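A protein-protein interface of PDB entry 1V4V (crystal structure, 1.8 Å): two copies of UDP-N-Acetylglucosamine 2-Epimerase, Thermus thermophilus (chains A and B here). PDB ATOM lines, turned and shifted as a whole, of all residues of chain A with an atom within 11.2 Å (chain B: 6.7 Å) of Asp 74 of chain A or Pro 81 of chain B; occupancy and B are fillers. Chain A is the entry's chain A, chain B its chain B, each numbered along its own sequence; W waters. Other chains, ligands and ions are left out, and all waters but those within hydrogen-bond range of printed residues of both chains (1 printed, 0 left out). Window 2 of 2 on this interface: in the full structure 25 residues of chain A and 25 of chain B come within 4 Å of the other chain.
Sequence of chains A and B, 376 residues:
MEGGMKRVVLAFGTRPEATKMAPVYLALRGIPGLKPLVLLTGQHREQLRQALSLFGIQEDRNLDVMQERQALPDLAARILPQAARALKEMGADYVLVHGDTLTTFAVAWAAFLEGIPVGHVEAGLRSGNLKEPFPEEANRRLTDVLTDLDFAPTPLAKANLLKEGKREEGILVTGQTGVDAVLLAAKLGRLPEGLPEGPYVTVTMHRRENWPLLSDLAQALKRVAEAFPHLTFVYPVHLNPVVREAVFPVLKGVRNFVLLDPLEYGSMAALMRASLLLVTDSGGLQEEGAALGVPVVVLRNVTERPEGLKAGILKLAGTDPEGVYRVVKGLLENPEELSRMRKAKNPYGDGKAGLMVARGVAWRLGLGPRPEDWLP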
ATOM      1  N   GLN A  43     -28.585 -18.590  33.086  1.00  0.00           N
ATOM      2  CA  GLN A  43     -27.471 -19.515  33.282  1.00  0.00           C
ATOM      3  C   GLN A  43     -27.783 -20.862  33.923  1.00  0.00           C
ATOM      4  O   GLN A  43     -27.001 -21.799  33.794  1.00  0.00           O
ATOM      5  CB  GLN A  43     -26.389 -18.846  34.132  1.00  0.00           C
ATOM      6  CG  GLN A  43     -25.812 -17.567  33.566  1.00  0.00           C
ATOM      7  CD  GLN A  43     -24.882 -16.880  34.552  1.00  0.00           C
ATOM      8  OE1 GLN A  43     -25.291 -16.510  35.652  1.00  0.00           O
ATOM      9  NE2 GLN A  43     -23.624 -16.708  34.161  1.00  0.00           N
ATOM     10  N   ASP A  64     -27.991 -20.099  24.795  1.00  0.00           N
ATOM     11  CA  ASP A  64     -26.723 -20.653  25.254  1.00  0.00           C
ATOM     12  C   ASP A  64     -25.961 -19.551  25.983  1.00  0.00           C
ATOM     13  O   ASP A  64     -25.402 -18.650  25.361  1.00  0.00           O
ATOM     14  CB  ASP A  64     -25.928 -21.174  24.054  1.00  0.00           C
ATOM     15  CG  ASP A  64     -24.686 -21.937  24.461  1.00  0.00           C
ATOM     16  OD1 ASP A  64     -24.179 -22.725  23.635  1.00  0.00           O
ATOM     17  OD2 ASP A  64     -24.209 -21.743  25.598  1.00  0.00           O
ATOM     18  N   VAL A  65     -25.950 -19.633  27.310  1.00  0.00           N
ATOM     19  CA  VAL A  65     -25.295 -18.625  28.136  1.00  0.00           C
ATOM     20  C   VAL A  65     -24.159 -19.185  28.987  1.00  0.00           C
ATOM     21  O   VAL A  65     -24.298 -20.235  29.610  1.00  0.00           O
ATOM     22  CB  VAL A  65     -26.330 -17.945  29.066  1.00  0.00           C
ATOM     23  CG1 VAL A  65     -25.655 -16.904  29.941  1.00  0.00           C
ATOM     24  CG2 VAL A  65     -27.432 -17.308  28.229  1.00  0.00           C
ATOM     25  N   MET A  66     -23.036 -18.471  29.011  1.00  0.00           N
ATOM     26  CA  MET A  66     -21.875 -18.891  29.793  1.00  0.00           C
ATOM     27  C   MET A  66     -22.222 -18.861  31.282  1.00  0.00           C
ATOM     28  O   MET A  66     -23.101 -18.115  31.706  1.00  0.00           O
ATOM     29  CB  MET A  66     -20.688 -17.947  29.540  1.00  0.00           C
ATOM     30  CG  MET A  66     -20.299 -17.745  28.079  1.00  0.00           C
ATOM     31  SD  MET A  66     -18.789 -16.520  27.853  1.00  0.00           S
ATOM     32  CE  MET A  66     -18.705 -15.795  29.638  1.00  0.00           C
ATOM     33  N   GLU A  68     -19.719 -18.439  33.650  1.00  0.00           N
ATOM     34  CA  GLU A  68     -18.765 -17.494  34.209  1.00  0.00           C
ATOM     35  C   GLU A  68     -19.226 -16.046  34.103  1.00  0.00           C
ATOM     36  O   GLU A  68     -19.983 -15.683  33.205  1.00  0.00           O
ATOM     37  CB  GLU A  68     -17.412 -17.640  33.508  1.00  0.00           C
ATOM     38  CG  GLU A  68     -17.503 -17.487  32.002  1.00  0.00           C
ATOM     39  CD  GLU A  68     -16.153 -17.304  31.338  1.00  0.00           C
ATOM     40  OE1 GLU A  68     -15.419 -16.372  31.729  1.00  0.00           O
ATOM     41  OE2 GLU A  68     -15.832 -18.083  30.419  1.00  0.00           O
ATOM     42  N   ARG A  69     -18.750 -15.229  35.036  1.00  0.00           N
ATOM     43  CA  ARG A  69     -19.062 -13.806  35.080  1.00  0.00           C
ATOM     44  C   ARG A  69     -18.556 -13.224  33.759  1.00  0.00           C
ATOM     45  O   ARG A  69     -17.586 -13.726  33.194  1.00  0.00           O
ATOM     46  CB  ARG A  69     -18.343 -13.181  36.279  1.00  0.00           C
ATOM     47  CG  ARG A  69     -18.654 -11.726  36.565  1.00  0.00           C
ATOM     48  CD  ARG A  69     -18.068 -11.308  37.917  1.00  0.00           C
ATOM     49  NE  ARG A  69     -16.739 -11.880  38.156  1.00  0.00           N
ATOM     50  CZ  ARG A  69     -16.515 -13.030  38.788  1.00  0.00           C
ATOM     51  NH1 ARG A  69     -15.274 -13.468  38.948  1.00  0.00           N
ATOM     52  NH2 ARG A  69     -17.528 -13.737  39.274  1.00  0.00           N
ATOM     53  N   GLN A  70     -19.205 -12.177  33.265  1.00  0.00           N
ATOM     54  CA  GLN A  70     -18.813 -11.592  31.988  1.00  0.00           C
ATOM     55  C   GLN A  70     -19.107 -10.092  31.904  1.00  0.00           C
ATOM     56  O   GLN A  70     -20.099  -9.616  32.451  1.00  0.00           O
ATOM     57  CB  GLN A  70     -19.545 -12.351  30.877  1.00  0.00           C
ATOM     58  CG  GLN A  70     -19.405 -11.811  29.479  1.00  0.00           C
ATOM     59  CD  GLN A  70     -19.984 -12.768  28.448  1.00  0.00           C
ATOM     60  OE1 GLN A  70     -21.094 -13.281  28.614  1.00  0.00           O
ATOM     61  NE2 GLN A  70     -19.237 -13.006  27.376  1.00  0.00           N
ATOM     62  N   ALA A  71     -18.234  -9.355  31.220  1.00  0.00           N
ATOM     63  CA  ALA A  71     -18.399  -7.910  31.054  1.00  0.00           C
ATOM     64  C   ALA A  71     -19.723  -7.637  30.349  1.00  0.00           C
ATOM     65  O   ALA A  71     -20.113  -8.369  29.443  1.00  0.00           O
ATOM     66  CB  ALA A  71     -17.242  -7.340  30.241  1.00  0.00           C
ATOM     67  N   LEU A  72     -20.405  -6.571  30.753  1.00  0.00           N
ATOM     68  CA  LEU A  72     -21.701  -6.244  30.174  1.00  0.00           C
ATOM     69  C   LEU A  72     -21.757  -6.161  28.644  1.00  0.00           C
ATOM     70  O   LEU A  72     -22.674  -6.704  28.032  1.00  0.00           O
ATOM     71  CB  LEU A  72     -22.239  -4.953  30.802  1.00  0.00           C
ATOM     72  CG  LEU A  72     -22.452  -5.072  32.317  1.00  0.00           C
ATOM     73  CD1 LEU A  72     -23.042  -3.787  32.868  1.00  0.00           C
ATOM     74  CD2 LEU A  72     -23.383  -6.246  32.609  1.00  0.00           C
ATOM     75  N   PRO A  73     -20.791  -5.475  28.003  1.00  0.00           N
ATOM     76  CA  PRO A  73     -20.857  -5.407  26.537  1.00  0.00           C
ATOM     77  C   PRO A  73     -20.766  -6.792  25.883  1.00  0.00           C
ATOM     78  O   PRO A  73     -21.439  -7.067  24.888  1.00  0.00           O
ATOM     79  CB  PRO A  73     -19.662  -4.531  26.173  1.00  0.00           C
ATOM     80  CG  PRO A  73     -19.544  -3.620  27.372  1.00  0.00           C
ATOM     81  CD  PRO A  73     -19.752  -4.574  28.527  1.00  0.00           C
ATOM     82  N   ASP A  74     -19.927  -7.656  26.444  1.00  0.00           N
ATOM     83  CA  ASP A  74     -19.764  -8.998  25.896  1.00  0.00           C
ATOM     84  C   ASP A  74     -21.015  -9.839  26.114  1.00  0.00           C
ATOM     85  O   ASP A  74     -21.407 -10.610  25.238  1.00  0.00           O
ATOM     86  CB  ASP A  74     -18.544  -9.676  26.517  1.00  0.00           C
ATOM     87  CG  ASP A  74     -17.256  -8.932  26.214  1.00  0.00           C
ATOM     88  OD1 ASP A  74     -16.903  -8.817  25.022  1.00  0.00           O
ATOM     89  OD2 ASP A  74     -16.601  -8.457  27.165  1.00  0.00           O
ATOM     90  N   LEU A  75     -21.649  -9.691  27.271  1.00  0.00           N
ATOM     91  CA  LEU A  75     -22.870 -10.443  27.542  1.00  0.00           C
ATOM     92  C   LEU A  75     -23.954 -10.058  26.545  1.00  0.00           C
ATOM     93  O   LEU A  75     -24.586 -10.922  25.943  1.00  0.00           O
ATOM     94  CB  LEU A  75     -23.384 -10.182  28.961  1.00  0.00           C
ATOM     95  CG  LEU A  75     -24.782 -10.772  29.200  1.00  0.00           C
ATOM     96  CD1 LEU A  75     -24.704 -12.297  29.123  1.00  0.00           C
ATOM     97  CD2 LEU A  75     -25.331 -10.326  30.544  1.00  0.00           C
ATOM     98  N   ALA A  76     -24.172  -8.757  26.371  1.00  0.00           N
ATOM     99  CA  ALA A  76     -25.192  -8.290  25.439  1.00  0.00           C
ATOM    100  C   ALA A  76     -24.931  -8.824  24.033  1.00  0.00           C
ATOM    101  O   ALA A  76     -25.859  -9.240  23.337  1.00  0.00           O
ATOM    102  CB  ALA A  76     -25.229  -6.756  25.415  1.00  0.00           C
ATOM    103  N   ALA A  77     -23.669  -8.804  23.615  1.00  0.00           N
ATOM    104  CA  ALA A  77     -23.301  -9.279  22.288  1.00  0.00           C
ATOM    105  C   ALA A  77     -23.560 -10.779  22.160  1.00  0.00           C
ATOM    106  O   ALA A  77     -23.916 -11.263  21.088  1.00  0.00           O
ATOM    107  CB  ALA A  77     -21.835  -8.978  22.016  1.00  0.00           C
ATOM    108  N   ARG A  78     -23.377 -11.500  23.259  1.00  0.00           N
ATOM    109  CA  ARG A  78     -23.588 -12.950  23.285  1.00  0.00           C
ATOM    110  C   ARG A  78     -25.075 -13.298  23.190  1.00  0.00           C
ATOM    111  O   ARG A  78     -25.462 -14.283  22.559  1.00  0.00           O
ATOM    112  CB  ARG A  78     -23.008 -13.532  24.580  1.00  0.00           C
ATOM    113  CG  ARG A  78     -23.288 -15.014  24.793  1.00  0.00           C
ATOM    114  CD  ARG A  78     -22.027 -15.842  24.640  1.00  0.00           C
ATOM    115  NE  ARG A  78     -22.302 -17.274  24.704  1.00  0.00           N
ATOM    116  CZ  ARG A  78     -21.413 -18.217  24.407  1.00  0.00           C
ATOM    117  NH1 ARG A  78     -20.188 -17.880  24.027  1.00  0.00           N
ATOM    118  NH2 ARG A  78     -21.752 -19.496  24.479  1.00  0.00           N
ATOM    119  N   ILE A  79     -25.906 -12.476  23.819  1.00  0.00           N
ATOM    120  CA  ILE A  79     -27.346 -12.699  23.829  1.00  0.00           C
ATOM    121  C   ILE A  79     -28.095 -12.276  22.568  1.00  0.00           C
ATOM    122  O   ILE A  79     -28.909 -13.025  22.039  1.00  0.00           O
ATOM    123  CB  ILE A  79     -28.005 -11.955  25.018  1.00  0.00           C
ATOM    124  CG1 ILE A  79     -27.482 -12.510  26.343  1.00  0.00           C
ATOM    125  CG2 ILE A  79     -29.527 -12.032  24.917  1.00  0.00           C
ATOM    126  CD1 ILE A  79     -27.778 -13.990  26.572  1.00  0.00           C
ATOM    127  N   LEU A  80     -27.817 -11.070  22.089  1.00  0.00           N
ATOM    128  CA  LEU A  80     -28.530 -10.513  20.948  1.00  0.00           C
ATOM    129  C   LEU A  80     -28.787 -11.373  19.704  1.00  0.00           C
ATOM    130  O   LEU A  80     -29.938 -11.562  19.316  1.00  0.00           O
ATOM    131  CB  LEU A  80     -27.867  -9.197  20.520  1.00  0.00           C
ATOM    132  CG  LEU A  80     -28.674  -8.342  19.540  1.00  0.00           C
ATOM    133  CD1 LEU A  80     -30.018  -7.977  20.168  1.00  0.00           C
ATOM    134  CD2 LEU A  80     -27.890  -7.073  19.198  1.00  0.00           C
ATOM    135  N   PRO A  81     -27.730 -11.904  19.069  1.00  0.00           N
ATOM    136  CA  PRO A  81     -27.935 -12.721  17.865  1.00  0.00           C
ATOM    137  C   PRO A  81     -28.735 -13.998  18.076  1.00  0.00           C
ATOM    138  O   PRO A  81     -29.667 -14.285  17.327  1.00  0.00           O
ATOM    139  CB  PRO A  81     -26.510 -13.016  17.391  1.00  0.00           C
ATOM    140  CG  PRO A  81     -25.704 -11.872  17.963  1.00  0.00           C
ATOM    141  CD  PRO A  81     -26.294 -11.748  19.346  1.00  0.00           C
ATOM    142  N   GLN A  82     -28.359 -14.778  19.079  1.00  0.00           N
ATOM    143  CA  GLN A  82     -29.060 -16.025  19.326  1.00  0.00           C
ATOM    144  C   GLN A  82     -30.494 -15.795  19.786  1.00  0.00           C
ATOM    145  O   GLN A  82     -31.351 -16.643  19.574  1.00  0.00           O
ATOM    146  CB  GLN A  82     -28.299 -16.880  20.342  1.00  0.00           C
ATOM    147  CG  GLN A  82     -28.202 -16.300  21.734  1.00  0.00           C
ATOM    148  CD  GLN A  82     -27.532 -17.263  22.693  1.00  0.00           C
ATOM    149  OE1 GLN A  82     -27.872 -18.450  22.737  1.00  0.00           O
ATOM    150  NE2 GLN A  82     -26.581 -16.761  23.468  1.00  0.00           N
ATOM    151  N   LEU A 102     -29.805  -6.753  31.830  1.00  0.00           N
ATOM    152  CA  LEU A 102     -29.200  -6.496  30.528  1.00  0.00           C
ATOM    153  C   LEU A 102     -29.757  -7.508  29.515  1.00  0.00           C
ATOM    154  O   LEU A 102     -30.054  -7.164  28.369  1.00  0.00           O
ATOM    155  CB  LEU A 102     -27.679  -6.643  30.632  1.00  0.00           C
ATOM    156  CG  LEU A 102     -26.823  -6.234  29.429  1.00  0.00           C
ATOM    157  CD1 LEU A 102     -26.891  -4.737  29.247  1.00  0.00           C
ATOM    158  CD2 LEU A 102     -25.380  -6.657  29.657  1.00  0.00           C
ATOM    159  N   THR A 103     -29.903  -8.758  29.947  1.00  0.00           N
ATOM    160  CA  THR A 103     -30.420  -9.801  29.066  1.00  0.00           C
ATOM    161  C   THR A 103     -31.837  -9.470  28.617  1.00  0.00           C
ATOM    162  O   THR A 103     -32.189  -9.679  27.458  1.00  0.00           O
ATOM    163  CB  THR A 103     -30.401 -11.175  29.761  1.00  0.00           C
ATOM    164  OG1 THR A 103     -29.050 -11.512  30.094  1.00  0.00           O
ATOM    165  CG2 THR A 103     -30.975 -12.259  28.841  1.00  0.00           C
ATOM    166  N   ALA A 106     -31.602  -6.938  25.912  1.00  0.00           N
ATOM    167  CA  ALA A 106     -31.016  -7.549  24.723  1.00  0.00           C
ATOM    168  C   ALA A 106     -32.067  -8.370  23.983  1.00  0.00           C
ATOM    169  O   ALA A 106     -32.113  -8.363  22.753  1.00  0.00           O
ATOM    170  CB  ALA A 106     -29.828  -8.425  25.108  1.00  0.00           C
ATOM    171  N   TRP A 109     -34.599  -5.991  22.368  1.00  0.00           N
ATOM    172  CA  TRP A 109     -34.032  -5.349  21.185  1.00  0.00           C
ATOM    173  C   TRP A 109     -33.985  -6.348  20.022  1.00  0.00           C
ATOM    174  O   TRP A 109     -34.234  -5.988  18.870  1.00  0.00           O
ATOM    175  CB  TRP A 109     -32.633  -4.802  21.497  1.00  0.00           C
ATOM    176  CG  TRP A 109     -32.084  -3.870  20.443  1.00  0.00           C
ATOM    177  CD1 TRP A 109     -32.798  -3.135  19.538  1.00  0.00           C
ATOM    178  CD2 TRP A 109     -30.706  -3.557  20.213  1.00  0.00           C
ATOM    179  NE1 TRP A 109     -31.948  -2.385  18.758  1.00  0.00           N
ATOM    180  CE2 TRP A 109     -30.660  -2.625  19.151  1.00  0.00           C
ATOM    181  CE3 TRP A 109     -29.505  -3.972  20.800  1.00  0.00           C
ATOM    182  CZ2 TRP A 109     -29.457  -2.102  18.665  1.00  0.00           C
ATOM    183  CZ3 TRP A 109     -28.308  -3.451  20.316  1.00  0.00           C
ATOM    184  CH2 TRP A 109     -28.296  -2.526  19.260  1.00  0.00           C
ATOM    185  N   PRO A 135     -26.627  -1.236  35.728  1.00  0.00           N
ATOM    186  CA  PRO A 135     -27.217  -0.562  34.566  1.00  0.00           C
ATOM    187  C   PRO A 135     -28.737  -0.735  34.468  1.00  0.00           C
ATOM    188  O   PRO A 135     -29.331  -0.440  33.431  1.00  0.00           O
ATOM    189  CB  PRO A 135     -26.504  -1.234  33.407  1.00  0.00           C
ATOM    190  CG  PRO A 135     -26.485  -2.667  33.867  1.00  0.00           C
ATOM    191  CD  PRO A 135     -26.083  -2.553  35.339  1.00  0.00           C
ATOM    192  N   ALA B  76     -24.921  -5.296  15.423  1.00  0.00           N
ATOM    193  CA  ALA B  76     -24.879  -4.726  16.765  1.00  0.00           C
ATOM    194  C   ALA B  76     -23.944  -5.527  17.668  1.00  0.00           C
ATOM    195  O   ALA B  76     -23.156  -4.957  18.418  1.00  0.00           O
ATOM    196  CB  ALA B  76     -26.284  -4.688  17.367  1.00  0.00           C
ATOM    197  N   ALA B  77     -24.039  -6.853  17.597  1.00  0.00           N
ATOM    198  CA  ALA B  77     -23.196  -7.718  18.409  1.00  0.00           C
ATOM    199  C   ALA B  77     -21.726  -7.577  18.046  1.00  0.00           C
ATOM    200  O   ALA B  77     -20.863  -7.722  18.901  1.00  0.00           O
ATOM    201  CB  ALA B  77     -23.632  -9.179  18.264  1.00  0.00           C
ATOM    202  N   ARG B  78     -21.442  -7.299  16.779  1.00  0.00           N
ATOM    203  CA  ARG B  78     -20.060  -7.145  16.340  1.00  0.00           C
ATOM    204  C   ARG B  78     -19.486  -5.805  16.797  1.00  0.00           C
ATOM    205  O   ARG B  78     -18.312  -5.716  17.154  1.00  0.00           O
ATOM    206  CB  ARG B  78     -19.970  -7.237  14.813  1.00  0.00           C
ATOM    207  CG  ARG B  78     -18.547  -7.404  14.288  1.00  0.00           C
ATOM    208  CD  ARG B  78     -18.488  -7.262  12.772  1.00  0.00           C
ATOM    209  NE  ARG B  78     -17.154  -7.544  12.247  1.00  0.00           N
ATOM    210  CZ  ARG B  78     -16.616  -8.757  12.188  1.00  0.00           C
ATOM    211  NH1 ARG B  78     -17.298  -9.809  12.617  1.00  0.00           N
ATOM    212  NH2 ARG B  78     -15.390  -8.919  11.705  1.00  0.00           N
ATOM    213  N   ILE B  79     -20.316  -4.765  16.794  1.00  0.00           N
ATOM    214  CA  ILE B  79     -19.865  -3.430  17.192  1.00  0.00           C
ATOM    215  C   ILE B  79     -19.663  -3.228  18.697  1.00  0.00           C
ATOM    216  O   ILE B  79     -18.647  -2.676  19.125  1.00  0.00           O
ATOM    217  CB  ILE B  79     -20.857  -2.335  16.708  1.00  0.00           C
ATOM    218  CG1 ILE B  79     -20.951  -2.334  15.180  1.00  0.00           C
ATOM    219  CG2 ILE B  79     -20.425  -0.965  17.225  1.00  0.00           C
ATOM    220  CD1 ILE B  79     -19.658  -1.981  14.465  1.00  0.00           C
ATOM    221  N   LEU B  80     -20.628  -3.683  19.494  1.00  0.00           N
ATOM    222  CA  LEU B  80     -20.602  -3.487  20.943  1.00  0.00           C
ATOM    223  C   LEU B  80     -19.303  -3.796  21.687  1.00  0.00           C
ATOM    224  O   LEU B  80     -18.721  -2.913  22.322  1.00  0.00           O
ATOM    225  CB  LEU B  80     -21.754  -4.267  21.600  1.00  0.00           C
ATOM    226  CG  LEU B  80     -22.795  -3.511  22.437  1.00  0.00           C
ATOM    227  CD1 LEU B  80     -23.591  -4.534  23.253  1.00  0.00           C
ATOM    228  CD2 LEU B  80     -22.133  -2.501  23.375  1.00  0.00           C
ATOM    229  N   PRO B  81     -18.829  -5.052  21.632  1.00  0.00           N
ATOM    230  CA  PRO B  81     -17.588  -5.384  22.343  1.00  0.00           C
ATOM    231  C   PRO B  81     -16.389  -4.585  21.849  1.00  0.00           C
ATOM    232  O   PRO B  81     -15.617  -4.054  22.650  1.00  0.00           O
ATOM    233  CB  PRO B  81     -17.425  -6.886  22.079  1.00  0.00           C
ATOM    234  CG  PRO B  81     -18.830  -7.347  21.799  1.00  0.00           C
ATOM    235  CD  PRO B  81     -19.356  -6.235  20.933  1.00  0.00           C
ATOM    236  N   GLN B  82     -16.243  -4.517  20.527  1.00  0.00           N
ATOM    237  CA  GLN B  82     -15.155  -3.779  19.874  1.00  0.00           C
ATOM    238  C   GLN B  82     -15.115  -2.338  20.342  1.00  0.00           C
ATOM    239  O   GLN B  82     -14.057  -1.788  20.662  1.00  0.00           O
ATOM    240  CB  GLN B  82     -15.382  -3.675  18.374  1.00  0.00           C
ATOM    241  CG  GLN B  82     -15.149  -4.855  17.525  1.00  0.00           C
ATOM    242  CD  GLN B  82     -15.080  -4.411  16.086  1.00  0.00           C
ATOM    243  OE1 GLN B  82     -14.112  -3.771  15.675  1.00  0.00           O
ATOM    244  NE2 GLN B  82     -16.120  -4.708  15.321  1.00  0.00           N
ATOM    245  N   ALA B  83     -16.288  -1.717  20.303  1.00  0.00           N
ATOM    246  CA  ALA B  83     -16.433  -0.326  20.684  1.00  0.00           C
ATOM    247  C   ALA B  83     -16.061  -0.096  22.130  1.00  0.00           C
ATOM    248  O   ALA B  83     -15.365   0.865  22.436  1.00  0.00           O
ATOM    249  CB  ALA B  83     -17.864   0.146  20.422  1.00  0.00           C
ATOM    250  N   ALA B  84     -16.522  -0.972  23.025  1.00  0.00           N
ATOM    251  CA  ALA B  84     -16.210  -0.815  24.437  1.00  0.00           C
ATOM    252  C   ALA B  84     -14.702  -0.885  24.650  1.00  0.00           C
ATOM    253  O   ALA B  84     -14.139  -0.083  25.395  1.00  0.00           O
ATOM    254  CB  ALA B  84     -16.909  -1.884  25.261  1.00  0.00           C
ATOM    255  N   ARG B  85     -14.046  -1.841  24.000  1.00  0.00           N
ATOM    256  CA  ARG B  85     -12.599  -1.969  24.142  1.00  0.00           C
ATOM    257  C   ARG B  85     -11.887  -0.762  23.541  1.00  0.00           C
ATOM    258  O   ARG B  85     -10.967  -0.210  24.141  1.00  0.00           O
ATOM    259  CB  ARG B  85     -12.086  -3.238  23.454  1.00  0.00           C
ATOM    260  CG  ARG B  85     -12.426  -4.533  24.166  1.00  0.00           C
ATOM    261  CD  ARG B  85     -11.547  -5.668  23.635  1.00  0.00           C
ATOM    262  NE  ARG B  85     -11.747  -5.905  22.208  1.00  0.00           N
ATOM    263  CZ  ARG B  85     -12.760  -6.603  21.700  1.00  0.00           C
ATOM    264  NH1 ARG B  85     -13.669  -7.140  22.503  1.00  0.00           N
ATOM    265  NH2 ARG B  85     -12.862  -6.764  20.388  1.00  0.00           N
ATOM    266  N   ALA B  86     -12.313  -0.346  22.356  1.00  0.00           N
ATOM    267  CA  ALA B  86     -11.674   0.796  21.707  1.00  0.00           C
ATOM    268  C   ALA B  86     -11.776   2.071  22.539  1.00  0.00           C
ATOM    269  O   ALA B  86     -10.791   2.802  22.688  1.00  0.00           O
ATOM    270  CB  ALA B  86     -12.280   1.022  20.325  1.00  0.00           C
ATOM    271  N   ALA B 110     -22.060   1.099  24.348  1.00  0.00           N
ATOM    272  CA  ALA B 110     -20.758   0.608  24.794  1.00  0.00           C
ATOM    273  C   ALA B 110     -20.151   1.635  25.753  1.00  0.00           C
ATOM    274  O   ALA B 110     -19.657   1.288  26.826  1.00  0.00           O
ATOM    275  CB  ALA B 110     -19.829   0.396  23.596  1.00  0.00           C
ATOM    276  N   LEU B 113     -22.011   1.646  29.098  1.00  0.00           N
ATOM    277  CA  LEU B 113     -21.692   0.467  29.893  1.00  0.00           C
ATOM    278  C   LEU B 113     -20.293   0.575  30.508  1.00  0.00           C
ATOM    279  O   LEU B 113     -20.009  -0.050  31.536  1.00  0.00           O
ATOM    280  CB  LEU B 113     -21.818  -0.800  29.024  1.00  0.00           C
ATOM    281  CG  LEU B 113     -23.267  -1.144  28.637  1.00  0.00           C
ATOM    282  CD1 LEU B 113     -23.311  -2.357  27.702  1.00  0.00           C
ATOM    283  CD2 LEU B 113     -24.072  -1.419  29.898  1.00  0.00           C
ATOM    284  N   GLU B 114     -19.432   1.381  29.886  1.00  0.00           N
ATOM    285  CA  GLU B 114     -18.069   1.587  30.376  1.00  0.00           C
ATOM    286  C   GLU B 114     -17.968   2.831  31.261  1.00  0.00           C
ATOM    287  O   GLU B 114     -16.881   3.185  31.716  1.00  0.00           O
ATOM    288  CB  GLU B 114     -17.081   1.721  29.211  1.00  0.00           C
ATOM    289  CG  GLU B 114     -16.962   0.485  28.327  1.00  0.00           C
ATOM    290  CD  GLU B 114     -16.422  -0.724  29.070  1.00  0.00           C
ATOM    291  OE1 GLU B 114     -16.576  -1.847  28.554  1.00  0.00           O
ATOM    292  OE2 GLU B 114     -15.837  -0.552  30.163  1.00  0.00           O
HETATM  293  O   HOH W   1     -13.965  -7.824  25.262  1.00  0.00           O
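Among the printed residues, pairs that only touch across the chains: Leu 72 of chain A with Leu 113 of chain B (3.9 Å), Pro 73 of chain A with Leu 80 of chain B (3.7 Å), Pro 73 of chain A with Ala 84 of chain B (3.8 Å), Pro 73 of chain A with Leu 113 of chain B (3.98 Å), Pro 73 of chain A with Glu 114 of chain B (3.7 Å), Asp 74 of chain A with Pro 81 of chain B (3.6 Å), Ala 76 of chain A with Leu 80 of chain B (3.5 Å), Ala 77 of chain A with Ala 77 of chain B (3.5 Å), Ala 77 of chain A with Pro 81 of chain B (3.4 Å), Leu 80 of chain A with Ala 76 of chain B (3.4 Å), Pro 81 of chain A with Ala 77 of chain B (3.4 Å) and Trp 109 of chain A with Ala 76 of chain B (3.5 Å).
Asp 74 of chain A touches just one residue of chain B: Pro 81 (3.6 Å). Pro 81 of chain B touches just these residues of chain A: Asp 74 (3.6 Å) and Ala 77 (3.4 Å). Ala 77 of chain B touches two residues of chain A. Leu 80 of chain B touches just these residues of chain A: Pro 73 (3.7 Å) and Ala 76 (3.5 Å). No residue of chain A comes within 4 Å of Ala 83 of chain B. Ala 84 of chain B touches just one residue of chain A: Pro 73. Of the printed residues of chain A, Leu 113 of chain B touches Leu 72 and Pro 73. Of the printed residues of chain B, Ala 77 of chain A touches Ala 77 and Pro 81. Printed residues of chain B within 4 Å of Pro 81 of chain A: Ala 77 (3.4 Å). Printed residues of chain B within 4 Å of Pro 73 of chain A: Leu 80 (3.7 Å), Ala 84 (3.8 Å), Leu 113 (3.98 Å) and Glu 114 (3.7 Å). Leu 75 of chain A touches none of the printed residues of chain B. Ala 71 of chain A touches none of the printed residues of chain B. The nearest residue of chain A that does not touch Pro 81 of chain B is Pro 73 of chain A (4.1 Å).
Of the 24 printed residues of chain A, 8 touch a printed residue of chain B. Of the 14 printed residues of chain B, 7 touch a printed residue of chain A. Among the printed residues, 12 pairs touch across the chains. Among the printed residues, no Asp or Glu carboxylate lies within 4 Å of a Lys or Arg side-chain nitrogen of the other chain.
Ala 76 of chain A touches Leu 80 of chain B, and with the chains exchanged Leu 80 of chain A touches Ala 76 of chain B. Ala 77 of chain B touches its own counterpart, Ala 77 of chain A. Ala 77 of chain A touches Pro 81 of chain B, and with the chains exchanged Pro 81 of chain A touches Ala 77 of chain B. Of the 12 pairs that touch across the chains among the printed residues, 5 have their exchanged pair printed and touching as well.
Water W1 lies within hydrogen-bond range of NH1 of Arg 85 of chain B (2.9 Å) and OD1 of Asp 74 of chain A (3.1 Å).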
